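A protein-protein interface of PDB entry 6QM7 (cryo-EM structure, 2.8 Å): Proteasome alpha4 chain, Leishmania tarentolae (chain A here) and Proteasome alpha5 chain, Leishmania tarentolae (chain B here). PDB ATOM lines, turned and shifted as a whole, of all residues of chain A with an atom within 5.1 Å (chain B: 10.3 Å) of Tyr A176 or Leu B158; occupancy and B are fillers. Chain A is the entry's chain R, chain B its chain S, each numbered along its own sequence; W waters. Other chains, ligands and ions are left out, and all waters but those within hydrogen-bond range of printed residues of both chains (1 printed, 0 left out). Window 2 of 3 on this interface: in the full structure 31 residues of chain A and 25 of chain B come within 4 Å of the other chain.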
ATOM      1  N   VAL A  35     -27.287  -5.243  -1.775  1.00  0.00           N
ATOM      2  CA  VAL A  35     -28.402  -4.615  -1.021  1.00  0.00           C
ATOM      3  C   VAL A  35     -29.192  -5.730  -0.342  1.00  0.00           C
ATOM      4  O   VAL A  35     -29.732  -6.591  -1.041  1.00  0.00           O
ATOM      5  CB  VAL A  35     -29.294  -3.752  -1.927  1.00  0.00           C
ATOM      6  CG1 VAL A  35     -30.288  -2.943  -1.107  1.00  0.00           C
ATOM      7  CG2 VAL A  35     -28.487  -2.826  -2.822  1.00  0.00           C
ATOM      8  N   LEU A  36     -29.218  -5.687   0.985  1.00  0.00           N
ATOM      9  CA  LEU A  36     -29.941  -6.618   1.877  1.00  0.00           C
ATOM     10  C   LEU A  36     -31.350  -6.068   2.080  1.00  0.00           C
ATOM     11  O   LEU A  36     -31.477  -4.875   2.419  1.00  0.00           O
ATOM     12  CB  LEU A  36     -29.184  -6.675   3.203  1.00  0.00           C
ATOM     13  CG  LEU A  36     -29.685  -7.690   4.222  1.00  0.00           C
ATOM     14  CD1 LEU A  36     -29.203  -9.087   3.865  1.00  0.00           C
ATOM     15  CD2 LEU A  36     -29.226  -7.300   5.622  1.00  0.00           C
ATOM     16  N   GLY A  37     -32.360  -6.912   1.873  1.00  0.00           N
ATOM     17  CA  GLY A  37     -33.777  -6.611   2.151  1.00  0.00           C
ATOM     18  C   GLY A  37     -34.323  -7.519   3.230  1.00  0.00           C
ATOM     19  O   GLY A  37     -33.535  -8.279   3.843  1.00  0.00           O
ATOM     20  N   ALA A 155     -19.901  -7.388   7.557  1.00  0.00           N
ATOM     21  CA  ALA A 155     -21.290  -7.524   7.069  1.00  0.00           C
ATOM     22  C   ALA A 155     -21.872  -6.132   6.907  1.00  0.00           C
ATOM     23  O   ALA A 155     -21.548  -5.268   7.724  1.00  0.00           O
ATOM     24  CB  ALA A 155     -22.134  -8.343   8.006  1.00  0.00           C
ATOM     25  N   TRP A 156     -22.688  -5.951   5.875  1.00  0.00           N
ATOM     26  CA  TRP A 156     -23.338  -4.664   5.520  1.00  0.00           C
ATOM     27  C   TRP A 156     -24.838  -4.863   5.330  1.00  0.00           C
ATOM     28  O   TRP A 156     -25.281  -6.016   5.145  1.00  0.00           O
ATOM     29  CB  TRP A 156     -22.708  -4.094   4.261  1.00  0.00           C
ATOM     30  CG  TRP A 156     -21.251  -3.814   4.413  1.00  0.00           C
ATOM     31  CD1 TRP A 156     -20.253  -4.715   4.651  1.00  0.00           C
ATOM     32  CD2 TRP A 156     -20.612  -2.538   4.287  1.00  0.00           C
ATOM     33  NE1 TRP A 156     -19.041  -4.082   4.707  1.00  0.00           N
ATOM     34  CE2 TRP A 156     -19.230  -2.747   4.485  1.00  0.00           C
ATOM     35  CE3 TRP A 156     -21.073  -1.253   4.005  1.00  0.00           C
ATOM     36  CZ2 TRP A 156     -18.308  -1.710   4.423  1.00  0.00           C
ATOM     37  CZ3 TRP A 156     -20.163  -0.217   3.963  1.00  0.00           C
ATOM     38  CH2 TRP A 156     -18.800  -0.446   4.174  1.00  0.00           C
ATOM     39  N   ARG A 157     -25.574  -3.764   5.410  1.00  0.00           N
ATOM     40  CA  ARG A 157     -26.998  -3.684   5.017  1.00  0.00           C
ATOM     41  C   ARG A 157     -27.038  -3.362   3.521  1.00  0.00           C
ATOM     42  O   ARG A 157     -27.936  -3.856   2.820  1.00  0.00           O
ATOM     43  CB  ARG A 157     -27.711  -2.679   5.924  1.00  0.00           C
ATOM     44  CG  ARG A 157     -28.005  -3.245   7.307  1.00  0.00           C
ATOM     45  CD  ARG A 157     -28.679  -2.281   8.266  1.00  0.00           C
ATOM     46  NE  ARG A 157     -27.949  -1.023   8.381  1.00  0.00           N
ATOM     47  CZ  ARG A 157     -28.461   0.194   8.205  1.00  0.00           C
ATOM     48  NH1 ARG A 157     -27.678   1.253   8.336  1.00  0.00           N
ATOM     49  NH2 ARG A 157     -29.741   0.365   7.904  1.00  0.00           N
ATOM     50  N   ALA A 158     -26.100  -2.554   3.055  1.00  0.00           N
ATOM     51  CA  ALA A 158     -25.860  -2.322   1.619  1.00  0.00           C
ATOM     52  C   ALA A 158     -24.394  -1.965   1.443  1.00  0.00           C
ATOM     53  O   ALA A 158     -23.844  -1.294   2.326  1.00  0.00           O
ATOM     54  CB  ALA A 158     -26.751  -1.222   1.106  1.00  0.00           C
ATOM     55  N   ILE A 169     -21.402   4.270  -1.613  1.00  0.00           N
ATOM     56  CA  ILE A 169     -21.695   4.018  -0.170  1.00  0.00           C
ATOM     57  C   ILE A 169     -22.242   5.303   0.459  1.00  0.00           C
ATOM     58  O   ILE A 169     -23.277   5.207   1.139  1.00  0.00           O
ATOM     59  CB  ILE A 169     -20.467   3.461   0.579  1.00  0.00           C
ATOM     60  CG1 ILE A 169     -20.192   2.012   0.161  1.00  0.00           C
ATOM     61  CG2 ILE A 169     -20.652   3.580   2.087  1.00  0.00           C
ATOM     62  CD1 ILE A 169     -18.862   1.445   0.617  1.00  0.00           C
ATOM     63  N   MET A 172     -25.694   5.648  -0.883  1.00  0.00           N
ATOM     64  CA  MET A 172     -26.575   4.576  -0.350  1.00  0.00           C
ATOM     65  C   MET A 172     -27.030   4.933   1.066  1.00  0.00           C
ATOM     66  O   MET A 172     -28.238   4.824   1.321  1.00  0.00           O
ATOM     67  CB  MET A 172     -25.868   3.223  -0.292  1.00  0.00           C
ATOM     68  CG  MET A 172     -25.895   2.448  -1.580  1.00  0.00           C
ATOM     69  SD  MET A 172     -24.954   0.920  -1.368  1.00  0.00           S
ATOM     70  CE  MET A 172     -25.284   0.113  -2.930  1.00  0.00           C
ATOM     71  N   GLU A 173     -26.112   5.336   1.953  1.00  0.00           N
ATOM     72  CA  GLU A 173     -26.410   5.459   3.408  1.00  0.00           C
ATOM     73  C   GLU A 173     -27.356   6.642   3.657  1.00  0.00           C
ATOM     74  O   GLU A 173     -27.988   6.659   4.730  1.00  0.00           O
ATOM     75  CB  GLU A 173     -25.137   5.455   4.267  1.00  0.00           C
ATOM     76  CG  GLU A 173     -24.162   6.610   4.077  1.00  0.00           C
ATOM     77  CD  GLU A 173     -22.799   6.355   4.723  1.00  0.00           C
ATOM     78  OE1 GLU A 173     -22.762   5.706   5.789  1.00  0.00           O
ATOM     79  OE2 GLU A 173     -21.773   6.794   4.158  1.00  0.00           O
ATOM     80  N   LYS A 174     -27.495   7.551   2.688  1.00  0.00           N
ATOM     81  CA  LYS A 174     -28.497   8.651   2.700  1.00  0.00           C
ATOM     82  C   LYS A 174     -29.908   8.085   2.477  1.00  0.00           C
ATOM     83  O   LYS A 174     -30.826   8.498   3.208  1.00  0.00           O
ATOM     84  CB  LYS A 174     -28.159   9.684   1.622  1.00  0.00           C
ATOM     85  CG  LYS A 174     -26.763  10.292   1.716  1.00  0.00           C
ATOM     86  CD  LYS A 174     -26.750  11.790   1.917  1.00  0.00           C
ATOM     87  CE  LYS A 174     -27.292  12.536   0.714  1.00  0.00           C
ATOM     88  NZ  LYS A 174     -26.836  13.945   0.690  1.00  0.00           N
ATOM     89  N   SER A 175     -30.072   7.169   1.517  1.00  0.00           N
ATOM     90  CA  SER A 175     -31.389   6.715   0.988  1.00  0.00           C
ATOM     91  C   SER A 175     -31.784   5.313   1.485  1.00  0.00           C
ATOM     92  O   SER A 175     -32.971   4.971   1.326  1.00  0.00           O
ATOM     93  CB  SER A 175     -31.421   6.791  -0.534  1.00  0.00           C
ATOM     94  OG  SER A 175     -30.123   6.651  -1.100  1.00  0.00           O
ATOM     95  N   TYR A 176     -30.869   4.522   2.058  1.00  0.00           N
ATOM     96  CA  TYR A 176     -31.128   3.095   2.400  1.00  0.00           C
ATOM     97  C   TYR A 176     -32.134   3.004   3.547  1.00  0.00           C
ATOM     98  O   TYR A 176     -31.930   3.677   4.570  1.00  0.00           O
ATOM     99  CB  TYR A 176     -29.860   2.334   2.804  1.00  0.00           C
ATOM    100  CG  TYR A 176     -30.112   0.883   3.144  1.00  0.00           C
ATOM    101  CD1 TYR A 176     -30.257  -0.070   2.149  1.00  0.00           C
ATOM    102  CD2 TYR A 176     -30.256   0.463   4.459  1.00  0.00           C
ATOM    103  CE1 TYR A 176     -30.519  -1.399   2.447  1.00  0.00           C
ATOM    104  CE2 TYR A 176     -30.518  -0.862   4.775  1.00  0.00           C
ATOM    105  CZ  TYR A 176     -30.647  -1.800   3.766  1.00  0.00           C
ATOM    106  OH  TYR A 176     -30.895  -3.108   4.066  1.00  0.00           O
ATOM    107  N   LYS A 177     -33.158   2.166   3.374  1.00  0.00           N
ATOM    108  CA  LYS A 177     -34.211   1.875   4.381  1.00  0.00           C
ATOM    109  C   LYS A 177     -34.138   0.391   4.736  1.00  0.00           C
ATOM    110  O   LYS A 177     -33.900  -0.418   3.823  1.00  0.00           O
ATOM    111  CB  LYS A 177     -35.592   2.238   3.831  1.00  0.00           C
ATOM    112  CG  LYS A 177     -36.091   3.639   4.169  1.00  0.00           C
ATOM    113  CD  LYS A 177     -37.289   4.090   3.333  1.00  0.00           C
ATOM    114  CE  LYS A 177     -38.368   3.032   3.144  1.00  0.00           C
ATOM    115  NZ  LYS A 177     -38.100   2.112   2.006  1.00  0.00           N
ATOM    116  N   ASP A 178     -34.380   0.065   6.008  1.00  0.00           N
ATOM    117  CA  ASP A 178     -34.074  -1.256   6.617  1.00  0.00           C
ATOM    118  C   ASP A 178     -34.932  -2.326   5.919  1.00  0.00           C
ATOM    119  O   ASP A 178     -34.374  -3.066   5.083  1.00  0.00           O
ATOM    120  CB  ASP A 178     -34.213  -1.195   8.146  1.00  0.00           C
ATOM    121  CG  ASP A 178     -33.188  -2.026   8.907  1.00  0.00           C
ATOM    122  OD1 ASP A 178     -32.008  -1.611   8.948  1.00  0.00           O
ATOM    123  OD2 ASP A 178     -33.577  -3.083   9.452  1.00  0.00           O
ATOM    124  N   MET A 180     -37.118  -3.811   3.206  1.00  0.00           N
ATOM    125  CA  MET A 180     -37.282  -3.556   1.749  1.00  0.00           C
ATOM    126  C   MET A 180     -37.836  -4.811   1.065  1.00  0.00           C
ATOM    127  O   MET A 180     -37.439  -5.936   1.438  1.00  0.00           O
ATOM    128  CB  MET A 180     -35.955  -3.162   1.091  1.00  0.00           C
ATOM    129  CG  MET A 180     -35.779  -1.658   0.873  1.00  0.00           C
ATOM    130  SD  MET A 180     -34.153  -1.245   0.164  1.00  0.00           S
ATOM    131  CE  MET A 180     -34.345   0.512  -0.136  1.00  0.00           C
ATOM    132  N   PHE A 188     -33.270  -0.206  -5.683  1.00  0.00           N
ATOM    133  CA  PHE A 188     -32.244   0.525  -4.894  1.00  0.00           C
ATOM    134  C   PHE A 188     -30.847   0.187  -5.406  1.00  0.00           C
ATOM    135  O   PHE A 188     -30.039   1.115  -5.554  1.00  0.00           O
ATOM    136  CB  PHE A 188     -32.341   0.177  -3.409  1.00  0.00           C
ATOM    137  CG  PHE A 188     -31.399   0.964  -2.539  1.00  0.00           C
ATOM    138  CD1 PHE A 188     -30.231   0.393  -2.062  1.00  0.00           C
ATOM    139  CD2 PHE A 188     -31.674   2.282  -2.219  1.00  0.00           C
ATOM    140  CE1 PHE A 188     -29.359   1.121  -1.269  1.00  0.00           C
ATOM    141  CE2 PHE A 188     -30.805   3.008  -1.418  1.00  0.00           C
ATOM    142  CZ  PHE A 188     -29.650   2.426  -0.945  1.00  0.00           C
ATOM    143  N   VAL B 154     -16.557   2.225  12.644  1.00  0.00           N
ATOM    144  CA  VAL B 154     -17.316   1.690  11.470  1.00  0.00           C
ATOM    145  C   VAL B 154     -17.100   2.623  10.279  1.00  0.00           C
ATOM    146  O   VAL B 154     -17.284   3.833  10.406  1.00  0.00           O
ATOM    147  CB  VAL B 154     -18.815   1.494  11.775  1.00  0.00           C
ATOM    148  CG1 VAL B 154     -19.060   0.211  12.556  1.00  0.00           C
ATOM    149  CG2 VAL B 154     -19.443   2.693  12.485  1.00  0.00           C
ATOM    150  N   PRO B 155     -16.692   2.104   9.094  1.00  0.00           N
ATOM    151  CA  PRO B 155     -16.412   2.957   7.938  1.00  0.00           C
ATOM    152  C   PRO B 155     -17.664   3.676   7.409  1.00  0.00           C
ATOM    153  O   PRO B 155     -17.516   4.736   6.828  1.00  0.00           O
ATOM    154  CB  PRO B 155     -15.842   1.996   6.880  1.00  0.00           C
ATOM    155  CG  PRO B 155     -16.364   0.628   7.283  1.00  0.00           C
ATOM    156  CD  PRO B 155     -16.486   0.678   8.791  1.00  0.00           C
ATOM    157  N   SER B 156     -18.848   3.102   7.637  1.00  0.00           N
ATOM    158  CA  SER B 156     -20.150   3.666   7.205  1.00  0.00           C
ATOM    159  C   SER B 156     -21.266   3.254   8.169  1.00  0.00           C
ATOM    160  O   SER B 156     -21.073   2.315   8.952  1.00  0.00           O
ATOM    161  CB  SER B 156     -20.472   3.250   5.793  1.00  0.00           C
ATOM    162  OG  SER B 156     -21.393   2.169   5.773  1.00  0.00           O
ATOM    163  N   THR B 157     -22.395   3.956   8.076  1.00  0.00           N
ATOM    164  CA  THR B 157     -23.664   3.679   8.801  1.00  0.00           C
ATOM    165  C   THR B 157     -24.220   2.320   8.370  1.00  0.00           C
ATOM    166  O   THR B 157     -24.850   1.651   9.209  1.00  0.00           O
ATOM    167  CB  THR B 157     -24.698   4.775   8.519  1.00  0.00           C
ATOM    168  OG1 THR B 157     -24.041   6.033   8.683  1.00  0.00           O
ATOM    169  CG2 THR B 157     -25.914   4.678   9.415  1.00  0.00           C
ATOM    170  N   LEU B 158     -23.987   1.935   7.112  1.00  0.00           N
ATOM    171  CA  LEU B 158     -24.531   0.688   6.505  1.00  0.00           C
ATOM    172  C   LEU B 158     -23.877  -0.567   7.079  1.00  0.00           C
ATOM    173  O   LEU B 158     -24.479  -1.637   6.928  1.00  0.00           O
ATOM    174  CB  LEU B 158     -24.345   0.733   4.992  1.00  0.00           C
ATOM    175  CG  LEU B 158     -25.243   1.748   4.301  1.00  0.00           C
ATOM    176  CD1 LEU B 158     -24.785   1.976   2.872  1.00  0.00           C
ATOM    177  CD2 LEU B 158     -26.696   1.303   4.347  1.00  0.00           C
ATOM    178  N   VAL B 159     -22.707  -0.459   7.695  1.00  0.00           N
ATOM    179  CA  VAL B 159     -22.036  -1.645   8.291  1.00  0.00           C
ATOM    180  C   VAL B 159     -22.911  -2.142   9.441  1.00  0.00           C
ATOM    181  O   VAL B 159     -23.307  -1.310  10.281  1.00  0.00           O
ATOM    182  CB  VAL B 159     -20.603  -1.348   8.762  1.00  0.00           C
ATOM    183  CG1 VAL B 159     -19.948  -2.592   9.343  1.00  0.00           C
ATOM    184  CG2 VAL B 159     -19.761  -0.772   7.634  1.00  0.00           C
ATOM    185  N   VAL B 160     -23.235  -3.435   9.424  1.00  0.00           N
ATOM    186  CA  VAL B 160     -23.767  -4.180  10.598  1.00  0.00           C
ATOM    187  C   VAL B 160     -22.671  -4.146  11.659  1.00  0.00           C
ATOM    188  O   VAL B 160     -21.670  -4.843  11.519  1.00  0.00           O
ATOM    189  CB  VAL B 160     -24.171  -5.613  10.197  1.00  0.00           C
ATOM    190  CG1 VAL B 160     -24.373  -6.542  11.388  1.00  0.00           C
ATOM    191  CG2 VAL B 160     -25.409  -5.588   9.318  1.00  0.00           C
ATOM    192  N   PRO B 161     -22.797  -3.328  12.731  1.00  0.00           N
ATOM    193  CA  PRO B 161     -21.670  -3.089  13.633  1.00  0.00           C
ATOM    194  C   PRO B 161     -21.258  -4.344  14.430  1.00  0.00           C
ATOM    195  O   PRO B 161     -20.075  -4.481  14.704  1.00  0.00           O
ATOM    196  CB  PRO B 161     -22.142  -1.916  14.512  1.00  0.00           C
ATOM    197  CG  PRO B 161     -23.656  -1.979  14.471  1.00  0.00           C
ATOM    198  CD  PRO B 161     -24.017  -2.614  13.144  1.00  0.00           C
ATOM    199  N   SER B 162     -22.197  -5.255  14.714  1.00  0.00           N
ATOM    200  CA  SER B 162     -21.931  -6.577  15.349  1.00  0.00           C
ATOM    201  C   SER B 162     -20.846  -7.354  14.592  1.00  0.00           C
ATOM    202  O   SER B 162     -20.108  -8.097  15.251  1.00  0.00           O
ATOM    203  CB  SER B 162     -23.191  -7.411  15.459  1.00  0.00           C
ATOM    204  OG  SER B 162     -23.591  -7.919  14.194  1.00  0.00           O
ATOM    205  N   SER B 163     -20.770  -7.194  13.266  1.00  0.00           N
ATOM    206  CA  SER B 163     -19.929  -8.004  12.341  1.00  0.00           C
ATOM    207  C   SER B 163     -18.447  -7.705  12.544  1.00  0.00           C
ATOM    208  O   SER B 163     -17.666  -8.664  12.567  1.00  0.00           O
ATOM    209  CB  SER B 163     -20.301  -7.776  10.894  1.00  0.00           C
ATOM    210  OG  SER B 163     -19.668  -6.614  10.359  1.00  0.00           O
ATOM    211  N   MET B 164     -18.087  -6.424  12.603  1.00  0.00           N
ATOM    212  CA  MET B 164     -16.687  -5.984  12.825  1.00  0.00           C
ATOM    213  C   MET B 164     -16.483  -5.776  14.330  1.00  0.00           C
ATOM    214  O   MET B 164     -16.415  -4.616  14.797  1.00  0.00           O
ATOM    215  CB  MET B 164     -16.324  -4.733  12.021  1.00  0.00           C
ATOM    216  CG  MET B 164     -17.304  -3.582  12.117  1.00  0.00           C
ATOM    217  SD  MET B 164     -16.435  -2.010  11.940  1.00  0.00           S
ATOM    218  CE  MET B 164     -15.512  -2.295  10.428  1.00  0.00           C
HETATM  219  O   HOH W   1     -26.066  -1.635  10.289  1.00  0.00           O
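The backbone carbonyl oxygen of Ala A155 is in hydrogen-bond range of the backbone NH of Val B160 (3.0 Å).
The backbone NH (N) of Ala A155 is in hydrogen-bond range of the side-chain hydroxyl (OG) of Ser B163 (2.9 Å).
O of Thr B157 is in hydrogen-bond range of NH1 of Arg A157 (3.0 Å).
The backbone NH (N) of Arg A157 lies within hydrogen-bond range of the backbone carbonyl oxygen (O) of Leu B158 (2.8 Å).
The backbone NH of Thr B157 sits at hydrogen-bond distance from the side-chain carboxylate of Glu A173 (2.9 Å).
N of Leu A36 lies within hydrogen-bond range of O of Arg A157 (2.9 Å).
O of Leu A36 is in hydrogen-bond range of OH of Tyr A176 (2.5 Å).
The backbone carbonyl oxygen (O) of Arg A157 lies within hydrogen-bond range of the side-chain hydroxyl (OH) of Tyr A176 (3.3 Å).
The side-chain carboxylate (OD1) of Asp A178 is in salt-bridge range of the guanidinium group (NH2) of Arg A157, 3.2 Å away.
OG of Ser B156 lies within hydrogen-bond range of N of Leu B158, 2.9 Å away.
The backbone carbonyl oxygen (O) of Val B160 sits at hydrogen-bond distance from the side-chain hydroxyl (OG) of Ser B163.
Among the printed residues, pairs that only touch across the chains: Ala A155 with Val B159 (3.5 Å), Trp A156 with Ser B156 (3.2 Å), Trp A156 with Leu B158 (3.5 Å), Trp A156 with Val B159 (3.6 Å), Ala A158 with Leu B158 (3.4 Å), Ile A169 with Ser B156 (3.7 Å), Ile A169 with Leu B158 (3.96 Å), Met A172 with Leu B158 (3.6 Å), Glu A173 with Ser B156 (3.4 Å), Glu A173 with Leu B158 (3.7 Å) and Tyr A176 with Leu B158 (3.6 Å).
Leu B158 touches just these residues of chain A: Trp A156 (3.5 Å), Arg A157 (2.8 Å), Ala A158 (3.4 Å), Ile A169 (3.96 Å), Met A172 (3.6 Å), Glu A173 (3.7 Å) and Tyr A176 (3.6 Å).
No residue of chain B comes within 4 Å of Gly A37.
Arg A157 touches two residues of chain B.
Of chain B, only Leu B158 comes within 4 Å of Ala A158.
Glu A173 touches three residues of chain B.
No residue of chain B comes within 4 Å of Ser A175.
No residue of chain B comes within 4 Å of Lys A177.
No residue of chain B comes within 4 Å of Asp A178.
Of the printed residues of chain B, Trp A156 touches Ser B156 (3.2 Å), Leu B158 (3.5 Å) and Val B159 (3.6 Å).
Of the printed residues of chain B, Ile A169 touches Ser B156 (3.7 Å) and Leu B158 (3.96 Å).
Of the printed residues of chain A, Val B159 touches Ala A155 and Trp A156.
Printed residues of chain A within 4 Å of Ser B156: Trp A156, Ile A169 and Glu A173.
Of the printed residues of chain B, Ala A155 touches Val B159 (3.5 Å), Val B160 (3.0 Å) and Ser B163 (2.9 Å).
Val B154 touches none of the printed residues of chain A.
Hydrophobic or aromatic side chains of chain B that line the printed part of chain A: Leu B158, Val B159 and Val B160.
Of the 17 printed residues of chain A, 8 touch a printed residue of chain B.
Hydrophobic or aromatic side chains of chain A within 4 Å of the printed part of chain B: Ala A155, Trp A156, Ile A169, Met A172 and Tyr A176.
Water W1 lies within hydrogen-bond range of the guanidinium group (NE) of Arg A157 (2.7 Å), the backbone carbonyl oxygen (O) of Val B159 (2.8 Å) and the backbone NH (N) of Val B160 (3.5 Å).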
